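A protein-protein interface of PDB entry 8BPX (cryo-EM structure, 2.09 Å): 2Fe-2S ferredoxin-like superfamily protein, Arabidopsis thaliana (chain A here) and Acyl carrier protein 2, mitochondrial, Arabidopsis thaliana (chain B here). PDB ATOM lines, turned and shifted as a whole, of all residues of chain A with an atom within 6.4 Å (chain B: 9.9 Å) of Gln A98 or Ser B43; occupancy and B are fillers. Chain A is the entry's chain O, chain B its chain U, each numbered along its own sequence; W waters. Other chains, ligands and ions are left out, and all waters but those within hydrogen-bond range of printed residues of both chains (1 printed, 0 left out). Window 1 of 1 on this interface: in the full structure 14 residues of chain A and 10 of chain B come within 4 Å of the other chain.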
ATOM      1  N   GLU A  96      12.034 -24.904  -8.866  1.00  0.00           N
ATOM      2  CA  GLU A  96      12.799 -25.187  -7.659  1.00  0.00           C
ATOM      3  C   GLU A  96      11.975 -24.935  -6.401  1.00  0.00           C
ATOM      4  O   GLU A  96      11.266 -23.932  -6.293  1.00  0.00           O
ATOM      5  CB  GLU A  96      14.066 -24.332  -7.630  1.00  0.00           C
ATOM      6  CG  GLU A  96      14.778 -24.325  -6.292  1.00  0.00           C
ATOM      7  CD  GLU A  96      16.142 -23.671  -6.354  1.00  0.00           C
ATOM      8  OE1 GLU A  96      16.418 -22.946  -7.332  1.00  0.00           O
ATOM      9  OE2 GLU A  96      16.937 -23.872  -5.415  1.00  0.00           O
ATOM     10  N   VAL A  97      12.072 -25.864  -5.447  1.00  0.00           N
ATOM     11  CA  VAL A  97      11.424 -25.740  -4.148  1.00  0.00           C
ATOM     12  C   VAL A  97      12.409 -26.147  -3.059  1.00  0.00           C
ATOM     13  O   VAL A  97      13.372 -26.876  -3.298  1.00  0.00           O
ATOM     14  CB  VAL A  97      10.143 -26.594  -4.045  1.00  0.00           C
ATOM     15  CG1 VAL A  97       9.059 -26.038  -4.946  1.00  0.00           C
ATOM     16  CG2 VAL A  97      10.446 -28.049  -4.380  1.00  0.00           C
ATOM     17  N   GLN A  98      12.142 -25.674  -1.845  1.00  0.00           N
ATOM     18  CA  GLN A  98      12.934 -26.018  -0.672  1.00  0.00           C
ATOM     19  C   GLN A  98      12.104 -26.880   0.267  1.00  0.00           C
ATOM     20  O   GLN A  98      10.980 -26.512   0.625  1.00  0.00           O
ATOM     21  CB  GLN A  98      13.419 -24.762   0.052  1.00  0.00           C
ATOM     22  CG  GLN A  98      14.682 -24.177  -0.531  1.00  0.00           C
ATOM     23  CD  GLN A  98      14.397 -23.180  -1.627  1.00  0.00           C
ATOM     24  OE1 GLN A  98      13.514 -22.335  -1.499  1.00  0.00           O
ATOM     25  NE2 GLN A  98      15.142 -23.275  -2.721  1.00  0.00           N
ATOM     26  N   ILE A  99      12.665 -28.017   0.670  1.00  0.00           N
ATOM     27  CA  ILE A  99      11.973 -29.005   1.486  1.00  0.00           C
ATOM     28  C   ILE A  99      12.857 -29.376   2.669  1.00  0.00           C
ATOM     29  O   ILE A  99      14.060 -29.606   2.506  1.00  0.00           O
ATOM     30  CB  ILE A  99      11.610 -30.259   0.662  1.00  0.00           C
ATOM     31  CG1 ILE A  99      10.817 -29.870  -0.590  1.00  0.00           C
ATOM     32  CG2 ILE A  99      10.823 -31.242   1.501  1.00  0.00           C
ATOM     33  CD1 ILE A  99      10.479 -31.029  -1.495  1.00  0.00           C
ATOM     34  N   ALA A 100      12.262 -29.434   3.857  1.00  0.00           N
ATOM     35  CA  ALA A 100      12.991 -29.824   5.055  1.00  0.00           C
ATOM     36  C   ALA A 100      13.370 -31.303   4.996  1.00  0.00           C
ATOM     37  O   ALA A 100      12.731 -32.111   4.317  1.00  0.00           O
ATOM     38  CB  ALA A 100      12.163 -29.539   6.309  1.00  0.00           C
ATOM     39  N   ASN A 128      22.111 -25.580  -2.877  1.00  0.00           N
ATOM     40  CA  ASN A 128      21.355 -25.639  -1.633  1.00  0.00           C
ATOM     41  C   ASN A 128      20.982 -27.087  -1.332  1.00  0.00           C
ATOM     42  O   ASN A 128      20.423 -27.784  -2.184  1.00  0.00           O
ATOM     43  CB  ASN A 128      20.106 -24.760  -1.732  1.00  0.00           C
ATOM     44  CG  ASN A 128      19.369 -24.616  -0.405  1.00  0.00           C
ATOM     45  OD1 ASN A 128      19.345 -25.528   0.419  1.00  0.00           O
ATOM     46  ND2 ASN A 128      18.763 -23.455  -0.198  1.00  0.00           N
ATOM     47  N   LYS A 129      21.287 -27.536  -0.113  1.00  0.00           N
ATOM     48  CA  LYS A 129      21.085 -28.936   0.240  1.00  0.00           C
ATOM     49  C   LYS A 129      19.615 -29.294   0.418  1.00  0.00           C
ATOM     50  O   LYS A 129      19.271 -30.477   0.352  1.00  0.00           O
ATOM     51  CB  LYS A 129      21.863 -29.277   1.511  1.00  0.00           C
ATOM     52  CG  LYS A 129      21.396 -28.530   2.747  1.00  0.00           C
ATOM     53  CD  LYS A 129      22.193 -28.935   3.969  1.00  0.00           C
ATOM     54  CE  LYS A 129      21.725 -28.187   5.207  1.00  0.00           C
ATOM     55  NZ  LYS A 129      22.502 -28.579   6.415  1.00  0.00           N
ATOM     56  N   HIS A 130      18.744 -28.313   0.640  1.00  0.00           N
ATOM     57  CA  HIS A 130      17.312 -28.556   0.749  1.00  0.00           C
ATOM     58  C   HIS A 130      16.555 -28.236  -0.534  1.00  0.00           C
ATOM     59  O   HIS A 130      15.322 -28.253  -0.532  1.00  0.00           O
ATOM     60  CB  HIS A 130      16.721 -27.756   1.910  1.00  0.00           C
ATOM     61  CG  HIS A 130      17.343 -28.061   3.235  1.00  0.00           C
ATOM     62  ND1 HIS A 130      18.336 -27.285   3.791  1.00  0.00           N
ATOM     63  CD2 HIS A 130      17.127 -29.075   4.107  1.00  0.00           C
ATOM     64  CE1 HIS A 130      18.694 -27.797   4.954  1.00  0.00           C
ATOM     65  NE2 HIS A 130      17.977 -28.884   5.168  1.00  0.00           N
ATOM     66  N   SER A 131      17.258 -27.948  -1.624  1.00  0.00           N
ATOM     67  CA  SER A 131      16.610 -27.587  -2.875  1.00  0.00           C
ATOM     68  C   SER A 131      16.272 -28.828  -3.692  1.00  0.00           C
ATOM     69  O   SER A 131      17.085 -29.746  -3.821  1.00  0.00           O
ATOM     70  CB  SER A 131      17.504 -26.648  -3.689  1.00  0.00           C
ATOM     71  OG  SER A 131      17.320 -25.302  -3.284  1.00  0.00           O
ATOM     72  N   ARG A 132      15.057 -28.849  -4.234  1.00  0.00           N
ATOM     73  CA  ARG A 132      14.619 -29.888  -5.153  1.00  0.00           C
ATOM     74  C   ARG A 132      13.983 -29.248  -6.376  1.00  0.00           C
ATOM     75  O   ARG A 132      13.324 -28.209  -6.283  1.00  0.00           O
ATOM     76  CB  ARG A 132      13.611 -30.854  -4.504  1.00  0.00           C
ATOM     77  CG  ARG A 132      14.121 -31.563  -3.263  1.00  0.00           C
ATOM     78  CD  ARG A 132      15.234 -32.541  -3.598  1.00  0.00           C
ATOM     79  NE  ARG A 132      14.902 -33.408  -4.723  1.00  0.00           N
ATOM     80  CZ  ARG A 132      14.894 -34.733  -4.672  1.00  0.00           C
ATOM     81  NH1 ARG A 132      15.213 -35.385  -3.565  1.00  0.00           N
ATOM     82  NH2 ARG A 132      14.573 -35.422  -5.763  1.00  0.00           N
ATOM     83  N   VAL A 147       5.525 -30.418   3.660  1.00  0.00           N
ATOM     84  CA  VAL A 147       5.612 -28.963   3.631  1.00  0.00           C
ATOM     85  C   VAL A 147       6.707 -28.568   2.653  1.00  0.00           C
ATOM     86  O   VAL A 147       7.806 -29.135   2.674  1.00  0.00           O
ATOM     87  CB  VAL A 147       5.882 -28.386   5.029  1.00  0.00           C
ATOM     88  CG1 VAL A 147       5.855 -26.866   4.974  1.00  0.00           C
ATOM     89  CG2 VAL A 147       4.847 -28.902   6.025  1.00  0.00           C
ATOM     90  N   VAL A 148       6.407 -27.603   1.792  1.00  0.00           N
ATOM     91  CA  VAL A 148       7.305 -27.188   0.726  1.00  0.00           C
ATOM     92  C   VAL A 148       7.390 -25.667   0.725  1.00  0.00           C
ATOM     93  O   VAL A 148       6.374 -24.981   0.862  1.00  0.00           O
ATOM     94  CB  VAL A 148       6.819 -27.726  -0.639  1.00  0.00           C
ATOM     95  CG1 VAL A 148       7.308 -26.859  -1.781  1.00  0.00           C
ATOM     96  CG2 VAL A 148       7.252 -29.177  -0.817  1.00  0.00           C
ATOM     97  N   ALA A 149       8.604 -25.143   0.591  1.00  0.00           N
ATOM     98  CA  ALA A 149       8.833 -23.710   0.496  1.00  0.00           C
ATOM     99  C   ALA A 149       9.123 -23.337  -0.953  1.00  0.00           C
ATOM    100  O   ALA A 149      10.025 -23.904  -1.577  1.00  0.00           O
ATOM    101  CB  ALA A 149       9.989 -23.279   1.400  1.00  0.00           C
ATOM    102  N   VAL A 150       8.355 -22.391  -1.483  1.00  0.00           N
ATOM    103  CA  VAL A 150       8.506 -21.926  -2.858  1.00  0.00           C
ATOM    104  C   VAL A 150       9.326 -20.637  -2.824  1.00  0.00           C
ATOM    105  O   VAL A 150       8.857 -19.635  -2.265  1.00  0.00           O
ATOM    106  CB  VAL A 150       7.146 -21.700  -3.530  1.00  0.00           C
ATOM    107  CG1 VAL A 150       7.322 -20.976  -4.861  1.00  0.00           C
ATOM    108  CG2 VAL A 150       6.420 -23.025  -3.714  1.00  0.00           C
ATOM    109  N   PRO A 151      10.531 -20.616  -3.386  1.00  0.00           N
ATOM    110  CA  PRO A 151      11.328 -19.384  -3.381  1.00  0.00           C
ATOM    111  C   PRO A 151      10.796 -18.384  -4.396  1.00  0.00           C
ATOM    112  O   PRO A 151       9.890 -18.664  -5.180  1.00  0.00           O
ATOM    113  CB  PRO A 151      12.731 -19.867  -3.750  1.00  0.00           C
ATOM    114  CG  PRO A 151      12.493 -21.085  -4.574  1.00  0.00           C
ATOM    115  CD  PRO A 151      11.223 -21.721  -4.070  1.00  0.00           C
ATOM    116  N   GLU A 152      11.376 -17.188  -4.360  1.00  0.00           N
ATOM    117  CA  GLU A 152      10.982 -16.147  -5.299  1.00  0.00           C
ATOM    118  C   GLU A 152      11.288 -16.589  -6.725  1.00  0.00           C
ATOM    119  O   GLU A 152      12.316 -17.214  -6.992  1.00  0.00           O
ATOM    120  CB  GLU A 152      11.706 -14.840  -4.972  1.00  0.00           C
ATOM    121  CG  GLU A 152      12.053 -13.988  -6.174  1.00  0.00           C
ATOM    122  CD  GLU A 152      12.506 -12.597  -5.780  1.00  0.00           C
ATOM    123  OE1 GLU A 152      12.550 -12.308  -4.566  1.00  0.00           O
ATOM    124  OE2 GLU A 152      12.820 -11.793  -6.683  1.00  0.00           O
ATOM    125  N   VAL B  40      28.028 -26.420   1.757  1.00  0.00           N
ATOM    126  CA  VAL B  40      26.727 -26.229   1.128  1.00  0.00           C
ATOM    127  C   VAL B  40      25.855 -25.353   2.023  1.00  0.00           C
ATOM    128  O   VAL B  40      26.080 -25.264   3.231  1.00  0.00           O
ATOM    129  CB  VAL B  40      26.048 -27.583   0.830  1.00  0.00           C
ATOM    130  CG1 VAL B  40      25.498 -28.205   2.106  1.00  0.00           C
ATOM    131  CG2 VAL B  40      24.958 -27.428  -0.227  1.00  0.00           C
ATOM    132  N   ARG B  41      24.866 -24.698   1.424  1.00  0.00           N
ATOM    133  CA  ARG B  41      23.970 -23.794   2.127  1.00  0.00           C
ATOM    134  C   ARG B  41      22.562 -24.371   2.142  1.00  0.00           C
ATOM    135  O   ARG B  41      22.089 -24.905   1.134  1.00  0.00           O
ATOM    136  CB  ARG B  41      23.964 -22.412   1.469  1.00  0.00           C
ATOM    137  CG  ARG B  41      22.910 -21.461   2.016  1.00  0.00           C
ATOM    138  CD  ARG B  41      22.471 -20.455   0.968  1.00  0.00           C
ATOM    139  NE  ARG B  41      21.799 -21.092  -0.159  1.00  0.00           N
ATOM    140  CZ  ARG B  41      22.357 -21.302  -1.343  1.00  0.00           C
ATOM    141  NH1 ARG B  41      23.603 -20.936  -1.595  1.00  0.00           N
ATOM    142  NH2 ARG B  41      21.646 -21.897  -2.298  1.00  0.00           N
ATOM    143  N   GLY B  42      21.902 -24.277   3.296  1.00  0.00           N
ATOM    144  CA  GLY B  42      20.559 -24.777   3.470  1.00  0.00           C
ATOM    145  C   GLY B  42      19.562 -23.659   3.738  1.00  0.00           C
ATOM    146  O   GLY B  42      19.913 -22.493   3.892  1.00  0.00           O
ATOM    147  N   SER B  43      18.289 -24.050   3.801  1.00  0.00           N
ATOM    148  CA  SER B  43      17.198 -23.106   3.973  1.00  0.00           C
ATOM    149  C   SER B  43      16.359 -23.336   5.220  1.00  0.00           C
ATOM    150  O   SER B  43      15.538 -22.475   5.553  1.00  0.00           O
ATOM    151  CB  SER B  43      16.270 -23.132   2.748  1.00  0.00           C
ATOM    152  OG  SER B  43      15.338 -24.189   2.845  1.00  0.00           O
ATOM    153  N   PHE B  44      16.526 -24.459   5.913  1.00  0.00           N
ATOM    154  CA  PHE B  44      15.740 -24.754   7.103  1.00  0.00           C
ATOM    155  C   PHE B  44      16.664 -25.038   8.274  1.00  0.00           C
ATOM    156  O   PHE B  44      17.685 -25.716   8.123  1.00  0.00           O
ATOM    157  CB  PHE B  44      14.811 -25.951   6.884  1.00  0.00           C
ATOM    158  CG  PHE B  44      13.945 -25.835   5.665  1.00  0.00           C
ATOM    159  CD1 PHE B  44      12.873 -24.961   5.640  1.00  0.00           C
ATOM    160  CD2 PHE B  44      14.199 -26.611   4.548  1.00  0.00           C
ATOM    161  CE1 PHE B  44      12.076 -24.858   4.518  1.00  0.00           C
ATOM    162  CE2 PHE B  44      13.404 -26.515   3.426  1.00  0.00           C
ATOM    163  CZ  PHE B  44      12.344 -25.637   3.409  1.00  0.00           C
ATOM    164  N   LEU B  45      16.299 -24.516   9.440  1.00  0.00           N
ATOM    165  CA  LEU B  45      16.984 -24.868  10.672  1.00  0.00           C
ATOM    166  C   LEU B  45      16.751 -26.337  11.004  1.00  0.00           C
ATOM    167  O   LEU B  45      15.707 -26.910  10.680  1.00  0.00           O
ATOM    168  CB  LEU B  45      16.494 -23.999  11.826  1.00  0.00           C
ATOM    169  CG  LEU B  45      17.275 -22.732  12.180  1.00  0.00           C
ATOM    170  CD1 LEU B  45      17.706 -21.971  10.938  1.00  0.00           C
ATOM    171  CD2 LEU B  45      16.432 -21.857  13.088  1.00  0.00           C
ATOM    172  N   ASP B  46      17.738 -26.946  11.654  1.00  0.00           N
ATOM    173  CA  ASP B  46      17.641 -28.352  12.017  1.00  0.00           C
ATOM    174  C   ASP B  46      16.543 -28.566  13.052  1.00  0.00           C
ATOM    175  O   ASP B  46      16.277 -27.708  13.898  1.00  0.00           O
ATOM    176  CB  ASP B  46      18.977 -28.862  12.558  1.00  0.00           C
ATOM    177  CG  ASP B  46      20.135 -28.541  11.640  1.00  0.00           C
ATOM    178  OD1 ASP B  46      19.965 -28.652  10.408  1.00  0.00           O
ATOM    179  OD2 ASP B  46      21.220 -28.184  12.148  1.00  0.00           O
ATOM    180  N   VAL B  50      15.932 -26.576  16.752  1.00  0.00           N
ATOM    181  CA  VAL B  50      14.697 -25.850  17.032  1.00  0.00           C
ATOM    182  C   VAL B  50      14.026 -26.416  18.277  1.00  0.00           C
ATOM    183  O   VAL B  50      13.484 -25.669  19.102  1.00  0.00           O
ATOM    184  CB  VAL B  50      13.769 -25.890  15.803  1.00  0.00           C
ATOM    185  CG1 VAL B  50      12.357 -25.502  16.182  1.00  0.00           C
ATOM    186  CG2 VAL B  50      14.299 -24.981  14.708  1.00  0.00           C
ATOM    187  N   PHE B 118       6.096 -26.107  13.365  1.00  0.00           N
ATOM    188  CA  PHE B 118       6.005 -24.867  12.603  1.00  0.00           C
ATOM    189  C   PHE B 118       7.388 -24.299  12.287  1.00  0.00           C
ATOM    190  O   PHE B 118       7.764 -24.168  11.117  1.00  0.00           O
ATOM    191  CB  PHE B 118       5.161 -23.845  13.361  1.00  0.00           C
ATOM    192  CG  PHE B 118       4.913 -22.595  12.584  1.00  0.00           C
ATOM    193  CD1 PHE B 118       4.150 -22.628  11.433  1.00  0.00           C
ATOM    194  CD2 PHE B 118       5.473 -21.393  12.977  1.00  0.00           C
ATOM    195  CE1 PHE B 118       3.932 -21.488  10.703  1.00  0.00           C
ATOM    196  CE2 PHE B 118       5.254 -20.248  12.251  1.00  0.00           C
ATOM    197  CZ  PHE B 118       4.482 -20.295  11.114  1.00  0.00           C
ATOM    198  N   ILE B 119       8.165 -23.958  13.322  1.00  0.00           N
ATOM    199  CA  ILE B 119       9.446 -23.290  13.065  1.00  0.00           C
ATOM    200  C   ILE B 119      10.436 -24.211  12.357  1.00  0.00           C
ATOM    201  O   ILE B 119      11.283 -23.736  11.593  1.00  0.00           O
ATOM    202  CB  ILE B 119      10.093 -22.665  14.328  1.00  0.00           C
ATOM    203  CG1 ILE B 119       9.084 -22.014  15.277  1.00  0.00           C
ATOM    204  CG2 ILE B 119      11.155 -21.647  13.946  1.00  0.00           C
ATOM    205  CD1 ILE B 119       8.596 -22.873  16.371  1.00  0.00           C
ATOM    206  N   ALA B 120      10.352 -25.527  12.569  1.00  0.00           N
ATOM    207  CA  ALA B 120      11.343 -26.426  11.990  1.00  0.00           C
ATOM    208  C   ALA B 120      11.253 -26.526  10.471  1.00  0.00           C
ATOM    209  O   ALA B 120      12.160 -27.091   9.854  1.00  0.00           O
ATOM    210  CB  ALA B 120      11.208 -27.823  12.599  1.00  0.00           C
ATOM    211  N   SER B 121      10.199 -26.000   9.851  1.00  0.00           N
ATOM    212  CA  SER B 121      10.064 -26.069   8.402  1.00  0.00           C
ATOM    213  C   SER B 121       9.878 -24.700   7.759  1.00  0.00           C
ATOM    214  O   SER B 121       9.744 -24.618   6.534  1.00  0.00           O
ATOM    215  CB  SER B 121       8.903 -26.992   8.017  1.00  0.00           C
ATOM    216  OG  SER B 121       7.665 -26.475   8.459  1.00  0.00           O
ATOM    217  N   HIS B 122       9.875 -23.625   8.544  1.00  0.00           N
ATOM    218  CA  HIS B 122       9.665 -22.292   7.999  1.00  0.00           C
ATOM    219  C   HIS B 122      10.981 -21.730   7.478  1.00  0.00           C
ATOM    220  O   HIS B 122      11.933 -21.594   8.254  1.00  0.00           O
ATOM    221  CB  HIS B 122       9.080 -21.367   9.048  1.00  0.00           C
ATOM    222  CG  HIS B 122       8.168 -20.326   8.487  1.00  0.00           C
ATOM    223  ND1 HIS B 122       8.631 -19.146   7.945  1.00  0.00           N
ATOM    224  CD2 HIS B 122       6.821 -20.294   8.361  1.00  0.00           C
ATOM    225  CE1 HIS B 122       7.607 -18.428   7.521  1.00  0.00           C
ATOM    226  NE2 HIS B 122       6.497 -19.101   7.761  1.00  0.00           N
ATOM    227  N   PRO B 123      11.078 -21.386   6.191  1.00  0.00           N
ATOM    228  CA  PRO B 123      12.360 -20.906   5.649  1.00  0.00           C
ATOM    229  C   PRO B 123      12.846 -19.612   6.274  1.00  0.00           C
ATOM    230  O   PRO B 123      14.061 -19.409   6.392  1.00  0.00           O
ATOM    231  CB  PRO B 123      12.056 -20.738   4.156  1.00  0.00           C
ATOM    232  CG  PRO B 123      10.597 -20.449   4.114  1.00  0.00           C
ATOM    233  CD  PRO B 123       9.981 -21.260   5.217  1.00  0.00           C
ATOM    234  N   GLN B 124      11.935 -18.728   6.689  1.00  0.00           N
ATOM    235  CA  GLN B 124      12.333 -17.472   7.310  1.00  0.00           C
ATOM    236  C   GLN B 124      12.978 -17.662   8.678  1.00  0.00           C
ATOM    237  O   GLN B 124      13.545 -16.702   9.211  1.00  0.00           O
ATOM    238  CB  GLN B 124      11.123 -16.542   7.438  1.00  0.00           C
ATOM    239  CG  GLN B 124      10.665 -15.929   6.123  1.00  0.00           C
ATOM    240  CD  GLN B 124       9.415 -15.085   6.280  1.00  0.00           C
ATOM    241  OE1 GLN B 124       8.632 -15.278   7.208  1.00  0.00           O
ATOM    242  NE2 GLN B 124       9.225 -14.138   5.367  1.00  0.00           N
ATOM    243  N   ALA B 125      12.905 -18.856   9.256  1.00  0.00           N
ATOM    244  CA  ALA B 125      13.515 -19.099  10.555  1.00  0.00           C
ATOM    245  C   ALA B 125      15.034 -19.001  10.468  1.00  0.00           C
ATOM    246  O   ALA B 125      15.644 -19.422   9.483  1.00  0.00           O
ATOM    247  CB  ALA B 125      13.109 -20.471  11.086  1.00  0.00           C
ATOM    248  N   LYS B 126      15.639 -18.434  11.506  1.00  0.00           N
ATOM    249  CA  LYS B 126      17.084 -18.247  11.555  1.00  0.00           C
ATOM    250  C   LYS B 126      17.643 -18.677  12.907  1.00  0.00           C
ATOM    251  O   LYS B 126      18.846 -18.899  13.050  1.00  0.00           O
ATOM    252  CB  LYS B 126      17.455 -16.786  11.282  1.00  0.00           C
ATOM    253  CG  LYS B 126      16.890 -16.219   9.990  1.00  0.00           C
ATOM    254  CD  LYS B 126      17.080 -14.712   9.922  1.00  0.00           C
ATOM    255  CE  LYS B 126      16.568 -14.032  11.180  1.00  0.00           C
ATOM    256  NZ  LYS B 126      15.252 -13.372  10.958  1.00  0.00           N
HETATM  257  O   HOH W   1       8.946 -25.521   3.796  1.00  0.00           O
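The side-chain hydroxyl (OG) of Ser A131 is in hydrogen-bond range of the side-chain amide nitrogen (NE2) of Gln A98 (3.0 Å). The backbone carbonyl oxygen (O) of Gln A98 lies within hydrogen-bond range of the backbone NH (N) of Ala A149 (2.7 Å). The backbone NH (N) of Ile A99 is in hydrogen-bond range of the backbone carbonyl oxygen (O) of His A130. The side-chain amide oxygen of Asn A128 sits at hydrogen-bond distance from the backbone NH of His A130 (2.9 Å). OE2 of Glu A96 lies within hydrogen-bond range of NE2 of Gln A98.
Hydrophobic or aromatic side chains of chain A within 4 Å of the printed part of chain B: Ala A100, His A130, Val A147 and Ala A149. Hydrophobic or aromatic side chains of chain B within 4 Å of the printed part of chain A: Val B40, Phe B44 and Pro B123. Among the printed residues, no Asp or Glu carboxylate lies within 4 Å of a Lys or Arg side-chain nitrogen of the other chain.
OD1 of Asn A128 sits close to O of Arg B41. N of Lys A129 sits at hydrogen-bond distance from O of Arg B41 (3.0 Å). A ring nitrogen (ND1) of His A130 is in hydrogen-bond range of the backbone NH (N) of Ser B43, 3.2 Å away.
CZ of Phe B44 touches O of Gln A98, at 3.2 Å. CE2 of Phe B44 touches C of Ile A99, 3.0 Å away. Phe B44 touches Ala A100 (CE2 to N, 3.2 Å). Asn A128 touches Gly B42 (OD1 to CA, 3.4 Å). Asn A128 touches Ser B43. Val B40 touches Lys A129 (CG2 to N, 3.7 Å). Gly B42 touches Lys A129 (CA to CG, 3.9 Å). His A130 touches Gly B42. CG of His A130 touches CD2 of Phe B44 (3.7 Å). Val A147 touches Ser B121 (CG1 to OG, 3.9 Å).
No residue of chain B comes within 4 Å of Val A97. Gln A98 touches two residues of chain B. Ile A99 touches one residue of chain B. Printed residues of chain B within 4 Å of His A130: Gly B42 (3.4 Å), Ser B43 (3.2 Å) and Phe B44 (3.7 Å). Of the printed residues of chain B, Val A147 touches Ser B121. Of chain B, only Phe B44 and Pro B123 come within 4 Å of Ala A149. Pro A151 touches none of the printed residues of chain B. Printed residues of chain A within 4 Å of Phe B44: Gln A98, Ile A99, Ala A100, His A130 and Ala A149. Of the printed residues of chain A, Ser B121 touches Val A147 (3.9 Å). Of the printed residues of chain A, Pro B123 touches Ala A149. The nearest residue of chain B that does not touch Gln A98 is Pro B123 (5.9 Å).
Water W1 lies within hydrogen-bond range of the backbone carbonyl oxygen (O) of Ser B121 (3.0 Å) and the backbone NH (N) of Ala A149 (3.2 Å).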
